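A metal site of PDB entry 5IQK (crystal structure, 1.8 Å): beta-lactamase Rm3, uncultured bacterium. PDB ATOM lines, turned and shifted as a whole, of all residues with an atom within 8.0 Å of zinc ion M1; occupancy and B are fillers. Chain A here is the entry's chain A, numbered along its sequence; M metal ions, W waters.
Zinc ion M1 is bound by water W1 (1.9 Å), NE2 of His 155 (2.0 Å), ND1 of His 79 (2.1 Å), NE2 of His 77 (2.1 Å) and water W2 (2.6 Å).
Zinc ion M1 has five donor atoms within binding distance.
Of the 21 residues printed, 3 come within 4 Å of zinc ion M1.
The nearest printed residue that does not touch zinc ion M1 is His 82 (4.2 Å).
OD2 of Asp 116 is in hydrogen-bond range of NE2 of His 79.
ND1 of His 155 is in hydrogen-bond range of O of Asn 182, 2.9 Å away.
OD1 of Asp 179 sits at hydrogen-bond distance from ND1 of His 77 (2.6 Å).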
ATOM      1  N   TRP A  10     -12.701  -6.439   0.297  1.00  0.00           N
ATOM      2  CA  TRP A  10     -13.816  -6.988  -0.472  1.00  0.00           C
ATOM      3  C   TRP A  10     -14.006  -8.491  -0.234  1.00  0.00           C
ATOM      4  O   TRP A  10     -15.137  -8.983  -0.216  1.00  0.00           O
ATOM      5  CB  TRP A  10     -13.623  -6.730  -1.959  1.00  0.00           C
ATOM      6  CG  TRP A  10     -13.858  -5.277  -2.368  1.00  0.00           C
ATOM      7  CD1 TRP A  10     -14.232  -4.239  -1.554  1.00  0.00           C
ATOM      8  CD2 TRP A  10     -13.713  -4.730  -3.677  1.00  0.00           C
ATOM      9  NE1 TRP A  10     -14.339  -3.067  -2.298  1.00  0.00           N
ATOM     10  CE2 TRP A  10     -14.031  -3.353  -3.602  1.00  0.00           C
ATOM     11  CE3 TRP A  10     -13.337  -5.255  -4.918  1.00  0.00           C
ATOM     12  CZ2 TRP A  10     -13.990  -2.511  -4.718  1.00  0.00           C
ATOM     13  CZ3 TRP A  10     -13.296  -4.418  -6.021  1.00  0.00           C
ATOM     14  CH2 TRP A  10     -13.627  -3.066  -5.910  1.00  0.00           C
ATOM     15  N   LEU A  31     -18.316  -8.403  -1.648  1.00  0.00           N
ATOM     16  CA  LEU A  31     -18.682  -8.965  -2.943  1.00  0.00           C
ATOM     17  C   LEU A  31     -19.795  -9.999  -2.783  1.00  0.00           C
ATOM     18  O   LEU A  31     -19.619 -10.968  -2.039  1.00  0.00           O
ATOM     19  CB  LEU A  31     -17.466  -9.635  -3.596  1.00  0.00           C
ATOM     20  CG  LEU A  31     -16.257  -8.744  -3.866  1.00  0.00           C
ATOM     21  CD1 LEU A  31     -15.056  -9.600  -4.239  1.00  0.00           C
ATOM     22  CD2 LEU A  31     -16.590  -7.752  -4.968  1.00  0.00           C
ATOM     23  N   SER A  76     -23.066 -11.301 -13.298  1.00  0.00           N
ATOM     24  CA  SER A  76     -23.565  -9.938 -13.388  1.00  0.00           C
ATOM     25  C   SER A  76     -22.741  -9.167 -14.434  1.00  0.00           C
ATOM     26  O   SER A  76     -23.271  -8.724 -15.448  1.00  0.00           O
ATOM     27  CB  SER A  76     -23.498  -9.248 -12.032  1.00  0.00           C
ATOM     28  OG  SER A  76     -22.180  -9.304 -11.510  1.00  0.00           O
ATOM     29  N   HIS A  77     -21.442  -9.013 -14.183  1.00  0.00           N
ATOM     30  CA  HIS A  77     -20.566  -8.443 -15.219  1.00  0.00           C
ATOM     31  C   HIS A  77     -19.139  -9.003 -15.142  1.00  0.00           C
ATOM     32  O   HIS A  77     -18.779  -9.691 -14.189  1.00  0.00           O
ATOM     33  CB  HIS A  77     -20.563  -6.909 -15.175  1.00  0.00           C
ATOM     34  CG  HIS A  77     -19.945  -6.288 -13.941  1.00  0.00           C
ATOM     35  ND1 HIS A  77     -20.622  -6.185 -12.742  1.00  0.00           N
ATOM     36  CD2 HIS A  77     -18.759  -5.652 -13.760  1.00  0.00           C
ATOM     37  CE1 HIS A  77     -19.861  -5.557 -11.859  1.00  0.00           C
ATOM     38  NE2 HIS A  77     -18.730  -5.227 -12.448  1.00  0.00           N
ATOM     39  N   GLY A  78     -18.333  -8.661 -16.151  1.00  0.00           N
ATOM     40  CA  GLY A  78     -17.082  -9.351 -16.408  1.00  0.00           C
ATOM     41  C   GLY A  78     -15.846  -8.910 -15.647  1.00  0.00           C
ATOM     42  O   GLY A  78     -14.745  -9.379 -15.908  1.00  0.00           O
ATOM     43  N   HIS A  79     -16.004  -7.965 -14.724  1.00  0.00           N
ATOM     44  CA  HIS A  79     -14.863  -7.577 -13.903  1.00  0.00           C
ATOM     45  C   HIS A  79     -14.389  -8.711 -13.019  1.00  0.00           C
ATOM     46  O   HIS A  79     -15.201  -9.537 -12.594  1.00  0.00           O
ATOM     47  CB  HIS A  79     -15.204  -6.365 -13.049  1.00  0.00           C
ATOM     48  CG  HIS A  79     -15.212  -5.072 -13.798  1.00  0.00           C
ATOM     49  ND1 HIS A  79     -15.938  -3.988 -13.374  1.00  0.00           N
ATOM     50  CD2 HIS A  79     -14.572  -4.683 -14.937  1.00  0.00           C
ATOM     51  CE1 HIS A  79     -15.741  -2.970 -14.205  1.00  0.00           C
ATOM     52  NE2 HIS A  79     -14.929  -3.370 -15.163  1.00  0.00           N
ATOM     53  N   ILE A  80     -13.093  -8.712 -12.744  1.00  0.00           N
ATOM     54  CA  ILE A  80     -12.465  -9.781 -11.974  1.00  0.00           C
ATOM     55  C   ILE A  80     -13.090 -10.018 -10.596  1.00  0.00           C
ATOM     56  O   ILE A  80     -13.051 -11.145 -10.089  1.00  0.00           O
ATOM     57  CB  ILE A  80     -10.928  -9.500 -11.816  1.00  0.00           C
ATOM     58  CG1 ILE A  80     -10.215 -10.683 -11.150  1.00  0.00           C
ATOM     59  CG2 ILE A  80     -10.686  -8.200 -11.041  1.00  0.00           C
ATOM     60  CD1 ILE A  80      -8.693 -10.654 -11.324  1.00  0.00           C
ATOM     61  N   ASP A  81     -13.674  -8.996  -9.987  1.00  0.00           N
ATOM     62  CA  ASP A  81     -14.221  -9.177  -8.644  1.00  0.00           C
ATOM     63  C   ASP A  81     -15.609  -9.813  -8.642  1.00  0.00           C
ATOM     64  O   ASP A  81     -16.186 -10.004  -7.560  1.00  0.00           O
ATOM     65  CB  ASP A  81     -14.266  -7.840  -7.874  1.00  0.00           C
ATOM     66  CG  ASP A  81     -15.037  -6.754  -8.616  1.00  0.00           C
ATOM     67  OD1 ASP A  81     -14.864  -6.662  -9.845  1.00  0.00           O
ATOM     68  OD2 ASP A  81     -15.802  -5.988  -7.973  1.00  0.00           O
ATOM     69  N   HIS A  82     -16.147 -10.142  -9.828  1.00  0.00           N
ATOM     70  CA  HIS A  82     -17.419 -10.886  -9.927  1.00  0.00           C
ATOM     71  C   HIS A  82     -17.232 -12.165 -10.753  1.00  0.00           C
ATOM     72  O   HIS A  82     -17.939 -13.162 -10.568  1.00  0.00           O
ATOM     73  CB  HIS A  82     -18.512  -9.982 -10.525  1.00  0.00           C
ATOM     74  CG  HIS A  82     -18.675  -8.691  -9.779  1.00  0.00           C
ATOM     75  ND1 HIS A  82     -19.445  -8.588  -8.637  1.00  0.00           N
ATOM     76  CD2 HIS A  82     -18.101  -7.480  -9.955  1.00  0.00           C
ATOM     77  CE1 HIS A  82     -19.364  -7.358  -8.162  1.00  0.00           C
ATOM     78  NE2 HIS A  82     -18.555  -6.660  -8.947  1.00  0.00           N
ATOM     79  N   ASP A 116     -14.201  -1.329 -21.856  1.00  0.00           N
ATOM     80  CA  ASP A 116     -14.439  -1.361 -20.424  1.00  0.00           C
ATOM     81  C   ASP A 116     -13.848  -0.119 -19.762  1.00  0.00           C
ATOM     82  O   ASP A 116     -12.712   0.273 -20.074  1.00  0.00           O
ATOM     83  CB  ASP A 116     -13.858  -2.627 -19.806  1.00  0.00           C
ATOM     84  CG  ASP A 116     -14.428  -2.918 -18.427  1.00  0.00           C
ATOM     85  OD1 ASP A 116     -15.248  -3.852 -18.325  1.00  0.00           O
ATOM     86  OD2 ASP A 116     -14.045  -2.231 -17.447  1.00  0.00           O
ATOM     87  N   GLN A 118     -12.560   0.066 -17.073  1.00  0.00           N
ATOM     88  CA  GLN A 118     -11.346  -0.329 -16.358  1.00  0.00           C
ATOM     89  C   GLN A 118     -10.398  -1.214 -17.176  1.00  0.00           C
ATOM     90  O   GLN A 118      -9.549  -1.917 -16.624  1.00  0.00           O
ATOM     91  CB  GLN A 118     -11.724  -0.999 -15.047  1.00  0.00           C
ATOM     92  CG  GLN A 118     -12.554  -0.072 -14.168  1.00  0.00           C
ATOM     93  CD  GLN A 118     -12.915  -0.668 -12.823  1.00  0.00           C
ATOM     94  OE1 GLN A 118     -14.089  -0.689 -12.444  1.00  0.00           O
ATOM     95  NE2 GLN A 118     -11.908  -1.135 -12.091  1.00  0.00           N
ATOM     96  N   LEU A 122      -7.030  -3.711 -14.646  1.00  0.00           N
ATOM     97  CA  LEU A 122      -7.390  -4.869 -13.812  1.00  0.00           C
ATOM     98  C   LEU A 122      -6.538  -6.071 -14.209  1.00  0.00           C
ATOM     99  O   LEU A 122      -6.128  -6.198 -15.361  1.00  0.00           O
ATOM    100  CB  LEU A 122      -8.882  -5.185 -13.939  1.00  0.00           C
ATOM    101  CG  LEU A 122      -9.878  -4.207 -13.290  1.00  0.00           C
ATOM    102  CD1 LEU A 122     -11.321  -4.547 -13.636  1.00  0.00           C
ATOM    103  CD2 LEU A 122      -9.688  -4.129 -11.790  1.00  0.00           C
ATOM    104  N   HIS A 155     -21.841   0.598 -16.024  1.00  0.00           N
ATOM    105  CA  HIS A 155     -20.624   0.365 -15.259  1.00  0.00           C
ATOM    106  C   HIS A 155     -19.674  -0.475 -16.118  1.00  0.00           C
ATOM    107  O   HIS A 155     -18.455  -0.293 -16.057  1.00  0.00           O
ATOM    108  CB  HIS A 155     -20.961  -0.313 -13.927  1.00  0.00           C
ATOM    109  CG  HIS A 155     -19.790  -0.843 -13.173  1.00  0.00           C
ATOM    110  ND1 HIS A 155     -19.021  -0.063 -12.329  1.00  0.00           N
ATOM    111  CD2 HIS A 155     -19.268  -2.095 -13.094  1.00  0.00           C
ATOM    112  CE1 HIS A 155     -18.069  -0.794 -11.788  1.00  0.00           C
ATOM    113  NE2 HIS A 155     -18.209  -2.045 -12.219  1.00  0.00           N
ATOM    114  N   THR A 156     -20.241  -1.388 -16.902  1.00  0.00           N
ATOM    115  CA  THR A 156     -19.544  -2.074 -18.007  1.00  0.00           C
ATOM    116  C   THR A 156     -20.539  -2.204 -19.158  1.00  0.00           C
ATOM    117  O   THR A 156     -21.746  -2.088 -18.936  1.00  0.00           O
ATOM    118  CB  THR A 156     -19.035  -3.480 -17.626  1.00  0.00           C
ATOM    119  OG1 THR A 156     -20.157  -4.352 -17.407  1.00  0.00           O
ATOM    120  CG2 THR A 156     -18.160  -3.449 -16.382  1.00  0.00           C
ATOM    121  N   ASP A 179     -26.967  -5.539 -10.720  1.00  0.00           N
ATOM    122  CA  ASP A 179     -25.581  -5.334 -11.065  1.00  0.00           C
ATOM    123  C   ASP A 179     -25.122  -3.955 -10.600  1.00  0.00           C
ATOM    124  O   ASP A 179     -25.928  -3.055 -10.355  1.00  0.00           O
ATOM    125  CB  ASP A 179     -25.370  -5.465 -12.580  1.00  0.00           C
ATOM    126  CG  ASP A 179     -23.898  -5.585 -12.932  1.00  0.00           C
ATOM    127  OD1 ASP A 179     -23.091  -5.932 -12.024  1.00  0.00           O
ATOM    128  OD2 ASP A 179     -23.542  -5.319 -14.093  1.00  0.00           O
ATOM    129  N   SER A 180     -23.813  -3.801 -10.480  1.00  0.00           N
ATOM    130  CA  SER A 180     -23.208  -2.478 -10.303  1.00  0.00           C
ATOM    131  C   SER A 180     -23.670  -1.528 -11.395  1.00  0.00           C
ATOM    132  O   SER A 180     -23.667  -1.905 -12.560  1.00  0.00           O
ATOM    133  CB  SER A 180     -21.680  -2.565 -10.350  1.00  0.00           C
ATOM    134  OG  SER A 180     -21.197  -3.439  -9.339  1.00  0.00           O
ATOM    135  N   ILE A 181     -24.065  -0.316 -11.008  1.00  0.00           N
ATOM    136  CA  ILE A 181     -24.393   0.740 -11.956  1.00  0.00           C
ATOM    137  C   ILE A 181     -23.691   2.035 -11.563  1.00  0.00           C
ATOM    138  O   ILE A 181     -24.141   3.143 -11.908  1.00  0.00           O
ATOM    139  CB  ILE A 181     -25.913   0.978 -12.034  1.00  0.00           C
ATOM    140  CG1 ILE A 181     -26.499   1.132 -10.632  1.00  0.00           C
ATOM    141  CG2 ILE A 181     -26.592  -0.180 -12.760  1.00  0.00           C
ATOM    142  CD1 ILE A 181     -27.945   1.561 -10.614  1.00  0.00           C
ATOM    143  N   ASN A 182     -22.573   1.896 -10.843  1.00  0.00           N
ATOM    144  CA  ASN A 182     -21.825   3.070 -10.427  1.00  0.00           C
ATOM    145  C   ASN A 182     -20.807   3.480 -11.494  1.00  0.00           C
ATOM    146  O   ASN A 182     -20.045   2.662 -12.021  1.00  0.00           O
ATOM    147  CB  ASN A 182     -21.144   2.824  -9.064  1.00  0.00           C
ATOM    148  CG  ASN A 182     -20.192   1.614  -9.051  1.00  0.00           C
ATOM    149  OD1 ASN A 182     -20.412   0.607  -9.722  1.00  0.00           O
ATOM    150  ND2 ASN A 182     -19.148   1.708  -8.242  1.00  0.00           N
ATOM    151  N   VAL A 184     -17.784   4.481 -12.104  1.00  0.00           N
ATOM    152  CA  VAL A 184     -16.397   4.526 -11.675  1.00  0.00           C
ATOM    153  C   VAL A 184     -15.565   3.863 -12.768  1.00  0.00           C
ATOM    154  O   VAL A 184     -16.086   3.066 -13.568  1.00  0.00           O
ATOM    155  CB  VAL A 184     -16.183   3.791 -10.343  1.00  0.00           C
ATOM    156  CG1 VAL A 184     -17.076   4.384  -9.276  1.00  0.00           C
ATOM    157  CG2 VAL A 184     -16.496   2.304 -10.512  1.00  0.00           C
ATOM    158  N   ALA A 222     -24.623  -6.285  -6.343  1.00  0.00           N
ATOM    159  CA  ALA A 222     -23.373  -6.992  -6.624  1.00  0.00           C
ATOM    160  C   ALA A 222     -22.302  -6.637  -5.602  1.00  0.00           C
ATOM    161  O   ALA A 222     -21.544  -7.510  -5.160  1.00  0.00           O
ATOM    162  CB  ALA A 222     -22.906  -6.679  -8.041  1.00  0.00           C
ATOM    163  N   HIS A 223     -22.243  -5.372  -5.213  1.00  0.00           N
ATOM    164  CA  HIS A 223     -21.470  -4.971  -4.028  1.00  0.00           C
ATOM    165  C   HIS A 223     -22.477  -4.757  -2.895  1.00  0.00           C
ATOM    166  O   HIS A 223     -23.264  -3.810  -2.962  1.00  0.00           O
ATOM    167  CB  HIS A 223     -20.633  -3.705  -4.299  1.00  0.00           C
ATOM    168  CG  HIS A 223     -19.447  -3.933  -5.178  1.00  0.00           C
ATOM    169  ND1 HIS A 223     -18.151  -3.957  -4.705  1.00  0.00           N
ATOM    170  CD2 HIS A 223     -19.366  -4.139  -6.521  1.00  0.00           C
ATOM    171  CE1 HIS A 223     -17.324  -4.184  -5.708  1.00  0.00           C
ATOM    172  NE2 HIS A 223     -18.034  -4.290  -6.819  1.00  0.00           N
HETATM  173 ZN    ZN M   1     -17.305  -3.844 -11.853  1.00  0.00          ZN
HETATM  174 ZN    ZN M   2     -17.424  -5.037  -8.599  1.00  0.00          ZN
HETATM  175  O   HOH W   1     -16.456  -4.003 -10.160  1.00  0.00           O
HETATM  176  O   HOH W   2     -18.643  -3.322  -9.708  1.00  0.00           O
